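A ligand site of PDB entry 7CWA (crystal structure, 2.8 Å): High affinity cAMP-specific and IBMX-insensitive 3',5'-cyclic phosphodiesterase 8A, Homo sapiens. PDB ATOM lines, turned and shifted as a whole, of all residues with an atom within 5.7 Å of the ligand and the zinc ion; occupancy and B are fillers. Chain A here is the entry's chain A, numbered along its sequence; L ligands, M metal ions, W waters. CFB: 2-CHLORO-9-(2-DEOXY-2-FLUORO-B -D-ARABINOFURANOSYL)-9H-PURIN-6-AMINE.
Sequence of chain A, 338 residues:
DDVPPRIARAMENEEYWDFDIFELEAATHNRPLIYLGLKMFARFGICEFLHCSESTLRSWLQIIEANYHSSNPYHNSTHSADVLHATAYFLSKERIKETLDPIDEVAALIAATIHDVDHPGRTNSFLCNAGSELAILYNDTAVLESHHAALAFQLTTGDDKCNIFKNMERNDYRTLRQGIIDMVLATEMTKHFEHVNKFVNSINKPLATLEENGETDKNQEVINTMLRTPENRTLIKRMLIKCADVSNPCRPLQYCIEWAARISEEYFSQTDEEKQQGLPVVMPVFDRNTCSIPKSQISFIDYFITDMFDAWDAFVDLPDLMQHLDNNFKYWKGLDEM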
ATOM      1  N   TYR A  74      23.208  -8.880  -8.320  1.00  0.00           N
ATOM      2  CA  TYR A  74      23.241  -7.935  -9.435  1.00  0.00           C
ATOM      3  C   TYR A  74      23.028  -8.635 -10.787  1.00  0.00           C
ATOM      4  O   TYR A  74      22.056  -8.343 -11.484  1.00  0.00           O
ATOM      5  CB  TYR A  74      24.577  -7.181  -9.443  1.00  0.00           C
ATOM      6  CG  TYR A  74      24.681  -6.100 -10.497  1.00  0.00           C
ATOM      7  CD1 TYR A  74      24.136  -4.827 -10.285  1.00  0.00           C
ATOM      8  CD2 TYR A  74      25.322  -6.340 -11.711  1.00  0.00           C
ATOM      9  CE1 TYR A  74      24.237  -3.832 -11.245  1.00  0.00           C
ATOM     10  CE2 TYR A  74      25.421  -5.359 -12.680  1.00  0.00           C
ATOM     11  CZ  TYR A  74      24.875  -4.102 -12.445  1.00  0.00           C
ATOM     12  OH  TYR A  74      24.979  -3.122 -13.406  1.00  0.00           O
ATOM     13  N   HIS A  75      23.916  -9.553 -11.136  1.00  0.00           N
ATOM     14  CA  HIS A  75      23.902 -10.194 -12.462  1.00  0.00           C
ATOM     15  C   HIS A  75      22.811 -11.248 -12.587  1.00  0.00           C
ATOM     16  O   HIS A  75      23.048 -12.446 -12.409  1.00  0.00           O
ATOM     17  CB  HIS A  75      25.286 -10.786 -12.804  1.00  0.00           C
ATOM     18  CG  HIS A  75      26.316  -9.754 -13.136  1.00  0.00           C
ATOM     19  ND1 HIS A  75      27.416  -9.508 -12.344  1.00  0.00           N
ATOM     20  CD2 HIS A  75      26.406  -8.891 -14.180  1.00  0.00           C
ATOM     21  CE1 HIS A  75      28.139  -8.546 -12.883  1.00  0.00           C
ATOM     22  NE2 HIS A  75      27.548  -8.164 -14.000  1.00  0.00           N
ATOM     23  N   HIS A  79      18.842  -7.216 -14.328  1.00  0.00           N
ATOM     24  CA  HIS A  79      19.947  -6.415 -14.849  1.00  0.00           C
ATOM     25  C   HIS A  79      19.936  -6.363 -16.379  1.00  0.00           C
ATOM     26  O   HIS A  79      20.073  -5.280 -16.947  1.00  0.00           O
ATOM     27  CB  HIS A  79      21.294  -6.947 -14.336  1.00  0.00           C
ATOM     28  CG  HIS A  79      22.481  -6.383 -15.050  1.00  0.00           C
ATOM     29  ND1 HIS A  79      22.682  -5.036 -15.198  1.00  0.00           N
ATOM     30  CD2 HIS A  79      23.522  -6.995 -15.659  1.00  0.00           C
ATOM     31  CE1 HIS A  79      23.803  -4.831 -15.871  1.00  0.00           C
ATOM     32  NE2 HIS A  79      24.330  -6.000 -16.165  1.00  0.00           N
ATOM     33  N   VAL A  83      19.516  -3.200 -18.866  1.00  0.00           N
ATOM     34  CA  VAL A  83      20.440  -2.920 -19.980  1.00  0.00           C
ATOM     35  C   VAL A  83      19.668  -2.880 -21.313  1.00  0.00           C
ATOM     36  O   VAL A  83      19.963  -2.036 -22.161  1.00  0.00           O
ATOM     37  CB  VAL A  83      21.595  -3.955 -20.030  1.00  0.00           C
ATOM     38  CG1 VAL A  83      22.455  -3.768 -21.278  1.00  0.00           C
ATOM     39  CG2 VAL A  83      22.455  -3.822 -18.782  1.00  0.00           C
ATOM     40  N   HIS A 115      23.856 -10.609 -22.886  1.00  0.00           N
ATOM     41  CA  HIS A 115      25.253 -10.209 -22.581  1.00  0.00           C
ATOM     42  C   HIS A 115      25.850 -10.744 -21.260  1.00  0.00           C
ATOM     43  O   HIS A 115      27.064 -10.840 -21.158  1.00  0.00           O
ATOM     44  CB  HIS A 115      25.422  -8.680 -22.645  1.00  0.00           C
ATOM     45  CG  HIS A 115      24.873  -7.948 -21.464  1.00  0.00           C
ATOM     46  ND1 HIS A 115      23.519  -7.757 -21.249  1.00  0.00           N
ATOM     47  CD2 HIS A 115      25.497  -7.347 -20.433  1.00  0.00           C
ATOM     48  CE1 HIS A 115      23.346  -7.079 -20.140  1.00  0.00           C
ATOM     49  NE2 HIS A 115      24.521  -6.813 -19.619  1.00  0.00           N
ATOM     50  N   ASP A 116      25.005 -11.066 -20.271  1.00  0.00           N
ATOM     51  CA  ASP A 116      25.453 -11.664 -19.003  1.00  0.00           C
ATOM     52  C   ASP A 116      24.695 -12.967 -18.671  1.00  0.00           C
ATOM     53  O   ASP A 116      24.462 -13.267 -17.507  1.00  0.00           O
ATOM     54  CB  ASP A 116      25.300 -10.663 -17.840  1.00  0.00           C
ATOM     55  CG  ASP A 116      26.298  -9.508 -17.904  1.00  0.00           C
ATOM     56  OD1 ASP A 116      27.464  -9.722 -18.300  1.00  0.00           O
ATOM     57  OD2 ASP A 116      25.921  -8.387 -17.521  1.00  0.00           O
ATOM     58  N   THR A 123      33.742 -12.696 -10.975  1.00  0.00           N
ATOM     59  CA  THR A 123      34.549 -12.053 -12.015  1.00  0.00           C
ATOM     60  C   THR A 123      35.348 -13.077 -12.829  1.00  0.00           C
ATOM     61  O   THR A 123      35.418 -14.254 -12.456  1.00  0.00           O
ATOM     62  CB  THR A 123      35.539 -11.041 -11.410  1.00  0.00           C
ATOM     63  OG1 THR A 123      36.394 -11.703 -10.471  1.00  0.00           O
ATOM     64  CG2 THR A 123      34.790  -9.914 -10.705  1.00  0.00           C
ATOM     65  N   THR A 187      31.920  -5.701 -23.882  1.00  0.00           N
ATOM     66  CA  THR A 187      31.630  -5.405 -22.464  1.00  0.00           C
ATOM     67  C   THR A 187      32.731  -5.836 -21.482  1.00  0.00           C
ATOM     68  O   THR A 187      32.657  -5.507 -20.299  1.00  0.00           O
ATOM     69  CB  THR A 187      30.303  -6.050 -22.015  1.00  0.00           C
ATOM     70  OG1 THR A 187      30.387  -7.470 -22.151  1.00  0.00           O
ATOM     71  CG2 THR A 187      29.132  -5.521 -22.833  1.00  0.00           C
ATOM     72  N   MET A 189      35.870  -5.600 -19.365  1.00  0.00           N
ATOM     73  CA  MET A 189      36.401  -4.370 -18.746  1.00  0.00           C
ATOM     74  C   MET A 189      37.913  -4.194 -18.893  1.00  0.00           C
ATOM     75  O   MET A 189      38.412  -3.078 -18.700  1.00  0.00           O
ATOM     76  CB  MET A 189      36.017  -4.303 -17.273  1.00  0.00           C
ATOM     77  CG  MET A 189      34.511  -4.299 -17.017  1.00  0.00           C
ATOM     78  SD  MET A 189      33.652  -2.850 -17.651  1.00  0.00           S
ATOM     79  CE  MET A 189      34.152  -1.600 -16.465  1.00  0.00           C
ATOM     80  N   ASP A 245      25.293  -0.959 -20.358  1.00  0.00           N
ATOM     81  CA  ASP A 245      25.692  -1.946 -19.357  1.00  0.00           C
ATOM     82  C   ASP A 245      25.907  -1.312 -17.983  1.00  0.00           C
ATOM     83  O   ASP A 245      25.376  -1.805 -16.984  1.00  0.00           O
ATOM     84  CB  ASP A 245      26.947  -2.694 -19.810  1.00  0.00           C
ATOM     85  CG  ASP A 245      27.337  -3.835 -18.882  1.00  0.00           C
ATOM     86  OD1 ASP A 245      26.437  -4.503 -18.328  1.00  0.00           O
ATOM     87  OD2 ASP A 245      28.548  -4.073 -18.708  1.00  0.00           O
ATOM     88  N   VAL A 246      26.666  -0.211 -17.948  1.00  0.00           N
ATOM     89  CA  VAL A 246      26.964   0.504 -16.690  1.00  0.00           C
ATOM     90  C   VAL A 246      26.278   1.881 -16.630  1.00  0.00           C
ATOM     91  O   VAL A 246      26.890   2.885 -16.248  1.00  0.00           O
ATOM     92  CB  VAL A 246      28.501   0.607 -16.438  1.00  0.00           C
ATOM     93  CG1 VAL A 246      29.081  -0.782 -16.221  1.00  0.00           C
ATOM     94  CG2 VAL A 246      29.232   1.310 -17.574  1.00  0.00           C
ATOM     95  N   ASN A 248      23.681   2.473 -14.614  1.00  0.00           N
ATOM     96  CA  ASN A 248      23.088   2.617 -13.278  1.00  0.00           C
ATOM     97  C   ASN A 248      23.482   3.866 -12.456  1.00  0.00           C
ATOM     98  O   ASN A 248      22.659   4.348 -11.670  1.00  0.00           O
ATOM     99  CB  ASN A 248      23.244   1.336 -12.424  1.00  0.00           C
ATOM    100  CG  ASN A 248      24.693   0.884 -12.243  1.00  0.00           C
ATOM    101  OD1 ASN A 248      25.425   1.442 -11.432  1.00  0.00           O
ATOM    102  ND2 ASN A 248      25.089  -0.132 -12.993  1.00  0.00           N
ATOM    103  N   PRO A 249      24.712   4.415 -12.644  1.00  0.00           N
ATOM    104  CA  PRO A 249      25.014   5.698 -11.989  1.00  0.00           C
ATOM    105  C   PRO A 249      24.298   6.904 -12.620  1.00  0.00           C
ATOM    106  O   PRO A 249      24.161   7.942 -11.959  1.00  0.00           O
ATOM    107  CB  PRO A 249      26.547   5.828 -12.158  1.00  0.00           C
ATOM    108  CG  PRO A 249      27.014   4.470 -12.543  1.00  0.00           C
ATOM    109  CD  PRO A 249      25.894   3.922 -13.367  1.00  0.00           C
ATOM    110  N   TRP A 259      21.068  -0.419  -7.346  1.00  0.00           N
ATOM    111  CA  TRP A 259      22.094  -1.073  -8.175  1.00  0.00           C
ATOM    112  C   TRP A 259      23.463  -1.112  -7.496  1.00  0.00           C
ATOM    113  O   TRP A 259      24.205  -2.078  -7.637  1.00  0.00           O
ATOM    114  CB  TRP A 259      22.235  -0.377  -9.543  1.00  0.00           C
ATOM    115  CG  TRP A 259      21.074  -0.577 -10.486  1.00  0.00           C
ATOM    116  CD1 TRP A 259      20.306   0.401 -11.063  1.00  0.00           C
ATOM    117  CD2 TRP A 259      20.540  -1.827 -10.954  1.00  0.00           C
ATOM    118  NE1 TRP A 259      19.343  -0.160 -11.860  1.00  0.00           N
ATOM    119  CE2 TRP A 259      19.457  -1.525 -11.819  1.00  0.00           C
ATOM    120  CE3 TRP A 259      20.875  -3.164 -10.727  1.00  0.00           C
ATOM    121  CZ2 TRP A 259      18.702  -2.518 -12.453  1.00  0.00           C
ATOM    122  CZ3 TRP A 259      20.128  -4.163 -11.365  1.00  0.00           C
ATOM    123  CH2 TRP A 259      19.054  -3.824 -12.213  1.00  0.00           C
ATOM    124  N   ALA A 260      23.794  -0.039  -6.764  1.00  0.00           N
ATOM    125  CA  ALA A 260      25.046   0.047  -5.997  1.00  0.00           C
ATOM    126  C   ALA A 260      25.126  -0.988  -4.875  1.00  0.00           C
ATOM    127  O   ALA A 260      26.174  -1.594  -4.675  1.00  0.00           O
ATOM    128  CB  ALA A 260      25.222   1.446  -5.433  1.00  0.00           C
ATOM    129  N   ILE A 263      25.434  -4.845  -6.589  1.00  0.00           N
ATOM    130  CA  ILE A 263      26.789  -5.141  -7.079  1.00  0.00           C
ATOM    131  C   ILE A 263      27.838  -5.190  -5.957  1.00  0.00           C
ATOM    132  O   ILE A 263      28.779  -5.979  -6.017  1.00  0.00           O
ATOM    133  CB  ILE A 263      27.244  -4.175  -8.212  1.00  0.00           C
ATOM    134  CG1 ILE A 263      28.508  -4.677  -8.924  1.00  0.00           C
ATOM    135  CG2 ILE A 263      27.476  -2.763  -7.691  1.00  0.00           C
ATOM    136  CD1 ILE A 263      28.414  -6.069  -9.499  1.00  0.00           C
ATOM    137  N   TYR A 267      30.272  -8.576  -4.580  1.00  0.00           N
ATOM    138  CA  TYR A 267      31.704  -8.587  -4.279  1.00  0.00           C
ATOM    139  C   TYR A 267      32.027  -9.163  -2.919  1.00  0.00           C
ATOM    140  O   TYR A 267      33.022  -9.889  -2.768  1.00  0.00           O
ATOM    141  CB  TYR A 267      32.309  -7.173  -4.344  1.00  0.00           C
ATOM    142  CG  TYR A 267      32.304  -6.522  -5.710  1.00  0.00           C
ATOM    143  CD1 TYR A 267      32.569  -7.252  -6.881  1.00  0.00           C
ATOM    144  CD2 TYR A 267      32.071  -5.154  -5.846  1.00  0.00           C
ATOM    145  CE1 TYR A 267      32.574  -6.646  -8.115  1.00  0.00           C
ATOM    146  CE2 TYR A 267      32.077  -4.541  -7.091  1.00  0.00           C
ATOM    147  CZ  TYR A 267      32.334  -5.289  -8.224  1.00  0.00           C
ATOM    148  OH  TYR A 267      32.339  -4.683  -9.458  1.00  0.00           O
ATOM    149  N   PHE A 286      36.801  -4.279  -1.748  1.00  0.00           N
ATOM    150  CA  PHE A 286      35.386  -4.648  -1.676  1.00  0.00           C
ATOM    151  C   PHE A 286      35.159  -5.822  -0.714  1.00  0.00           C
ATOM    152  O   PHE A 286      34.852  -6.938  -1.139  1.00  0.00           O
ATOM    153  CB  PHE A 286      34.851  -4.981  -3.081  1.00  0.00           C
ATOM    154  CG  PHE A 286      35.039  -3.868  -4.078  1.00  0.00           C
ATOM    155  CD1 PHE A 286      35.967  -3.975  -5.110  1.00  0.00           C
ATOM    156  CD2 PHE A 286      34.298  -2.689  -3.985  1.00  0.00           C
ATOM    157  CE1 PHE A 286      36.149  -2.956  -6.034  1.00  0.00           C
ATOM    158  CE2 PHE A 286      34.477  -1.664  -4.897  1.00  0.00           C
ATOM    159  CZ  PHE A 286      35.398  -1.802  -5.925  1.00  0.00           C
ATOM    160  N   SER A 296      33.376   3.849  -2.459  1.00  0.00           N
ATOM    161  CA  SER A 296      33.620   2.893  -3.547  1.00  0.00           C
ATOM    162  C   SER A 296      32.961   3.324  -4.856  1.00  0.00           C
ATOM    163  O   SER A 296      33.576   3.211  -5.919  1.00  0.00           O
ATOM    164  CB  SER A 296      33.118   1.492  -3.162  1.00  0.00           C
ATOM    165  OG  SER A 296      33.971   0.899  -2.201  1.00  0.00           O
ATOM    166  N   GLN A 297      31.729   3.811  -4.769  1.00  0.00           N
ATOM    167  CA  GLN A 297      30.988   4.296  -5.952  1.00  0.00           C
ATOM    168  C   GLN A 297      31.621   5.532  -6.592  1.00  0.00           C
ATOM    169  O   GLN A 297      31.584   5.683  -7.809  1.00  0.00           O
ATOM    170  CB  GLN A 297      29.522   4.578  -5.595  1.00  0.00           C
ATOM    171  CG  GLN A 297      28.701   3.337  -5.262  1.00  0.00           C
ATOM    172  CD  GLN A 297      28.597   2.350  -6.409  1.00  0.00           C
ATOM    173  OE1 GLN A 297      28.642   2.734  -7.582  1.00  0.00           O
ATOM    174  NE2 GLN A 297      28.460   1.072  -6.091  1.00  0.00           N
ATOM    175  N   PHE A 300      34.579   4.252  -8.607  1.00  0.00           N
ATOM    176  CA  PHE A 300      34.080   3.587  -9.822  1.00  0.00           C
ATOM    177  C   PHE A 300      33.646   4.595 -10.895  1.00  0.00           C
ATOM    178  O   PHE A 300      33.939   4.403 -12.077  1.00  0.00           O
ATOM    179  CB  PHE A 300      32.918   2.648  -9.486  1.00  0.00           C
ATOM    180  CG  PHE A 300      32.341   1.939 -10.680  1.00  0.00           C
ATOM    181  CD1 PHE A 300      33.031   0.895 -11.284  1.00  0.00           C
ATOM    182  CD2 PHE A 300      31.119   2.328 -11.216  1.00  0.00           C
ATOM    183  CE1 PHE A 300      32.501   0.237 -12.390  1.00  0.00           C
ATOM    184  CE2 PHE A 300      30.586   1.684 -12.321  1.00  0.00           C
ATOM    185  CZ  PHE A 300      31.281   0.640 -12.916  1.00  0.00           C
HETATM  186  O5' CFB L   1      30.725  -3.531 -17.088  1.00  0.00           O
HETATM  187  C5' CFB L   1      30.335  -4.515 -16.139  1.00  0.00           C
HETATM  188  C4' CFB L   1      31.201  -4.488 -14.905  1.00  0.00           C
HETATM  189  O4' CFB L   1      30.916  -3.273 -14.162  1.00  0.00           O
HETATM  190  C3' CFB L   1      31.001  -5.650 -13.935  1.00  0.00           C
HETATM  191  O3' CFB L   1      32.246  -6.205 -13.525  1.00  0.00           O
HETATM  192  C2' CFB L   1      30.275  -5.019 -12.757  1.00  0.00           C
HETATM  193  F   CFB L   1      28.893  -5.101 -12.959  1.00  0.00           F
HETATM  194  C1' CFB L   1      30.748  -3.578 -12.795  1.00  0.00           C
HETATM  195  N9  CFB L   1      29.810  -2.607 -12.235  1.00  0.00           N
HETATM  196  C8  CFB L   1      28.619  -2.199 -12.766  1.00  0.00           C
HETATM  197  N7  CFB L   1      28.013  -1.263 -12.082  1.00  0.00           N
HETATM  198  C5  CFB L   1      28.867  -1.030 -11.015  1.00  0.00           C
HETATM  199  C4  CFB L   1      29.980  -1.854 -11.089  1.00  0.00           C
HETATM  200  N3  CFB L   1      31.005  -1.892 -10.229  1.00  0.00           N
HETATM  201  C2  CFB L   1      30.838  -1.000  -9.263  1.00  0.00           C
HETATM  202 CL   CFB L   1      32.119  -0.941  -8.101  1.00  0.00          CL
HETATM  203  N1  CFB L   1      29.845  -0.139  -9.050  1.00  0.00           N
HETATM  204  C6  CFB L   1      28.826  -0.126  -9.936  1.00  0.00           C
HETATM  205  N6  CFB L   1      27.845   0.754  -9.752  1.00  0.00           N
HETATM  206 ZN    ZN M   1      26.871  -6.537 -17.909  1.00  0.00          ZN
HETATM  207 MG    MG M   2      30.526  -8.411 -18.739  1.00  0.00          MG
HETATM  208  O   HOH W   1      29.064  -7.021 -18.898  1.00  0.00           O
HETATM  209  O   HOH W   2      30.888  -2.913 -20.242  1.00  0.00           O
HETATM  210  O   HOH W   3      26.721  -3.880 -15.378  1.00  0.00           O
HETATM  211  O   HOH W   4      33.070  -7.037 -16.003  1.00  0.00           O
HETATM  212  O   HOH W   5      27.871  -6.537 -16.165  1.00  0.00           O
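Water W1 lies within hydrogen-bond range of OD2 of Asp 245 (3.0 Å) and OD1 of Asp 116 (3.2 Å).
Water W3 lies within hydrogen-bond range of OH of Tyr 74 (2.7 Å), O of Asp 245 (2.9 Å) and NE2 of His 79 (3.3 Å).
The side-chain carboxylate (OD2) of Asp 116 sits close to a ring nitrogen (NE2) of His 115 (3.0 Å).
The side-chain carboxylate (OD2) of Asp 116 sits close to a ring nitrogen (NE2) of His 79, at 3.2 Å.
OD1 of Asp 245 lies close to NE2 of His 115.
OD1 of Asp 245 sits close to NE2 of His 79 (3.4 Å).
The side-chain hydroxyl (OH) of Tyr 74 sits at hydrogen-bond distance from the side-chain amide nitrogen (ND2) of Asn 248, 3.0 Å away.
ND1 of His 79 sits close to OH of Tyr 74.
His 79 touches the zinc ion.
His 115 touches the zinc ion (NE2 to ZN, 2.9 Å).
Water W5 binds the zinc ion, 2.0 Å away.
OD2 of Asp 116 is bound to the zinc ion (2.1 Å).
OD1 of Asp 245 is bound to the zinc ion (2.1 Å).
Water W1 binds the zinc ion (2.5 Å).
The side-chain carboxylate of Asp 245 is in hydrogen-bond range of an oxygen (O5') of the ligand.
The side-chain amide oxygen (OD1) of Asn 248 lies within hydrogen-bond range of a nitrogen (N6) of the ligand, at 3.0 Å.
OE1 of Gln 297 is in hydrogen-bond range of N6 of the ligand, at 3.0 Å.
The side-chain sulfur of Met 189 is in hydrogen-bond range of an oxygen (O5') of the ligand, at 3.1 Å.
The side-chain hydroxyl (OH) of Tyr 267 sits at hydrogen-bond distance from a nitrogen (N3) of the ligand.
Residues that only touch the ligand: Val 246, Phe 300, Tyr 74, His 75 and Ile 263.
Ten residues have an atom within 4 Å of the ligand: Tyr 74, His 75, Met 189, Asp 245, Val 246, Asn 248, Ile 263, Tyr 267, Gln 297 and Phe 300.
Along chain A the residues within 4 Å of the ligand span positions 74 to 300.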
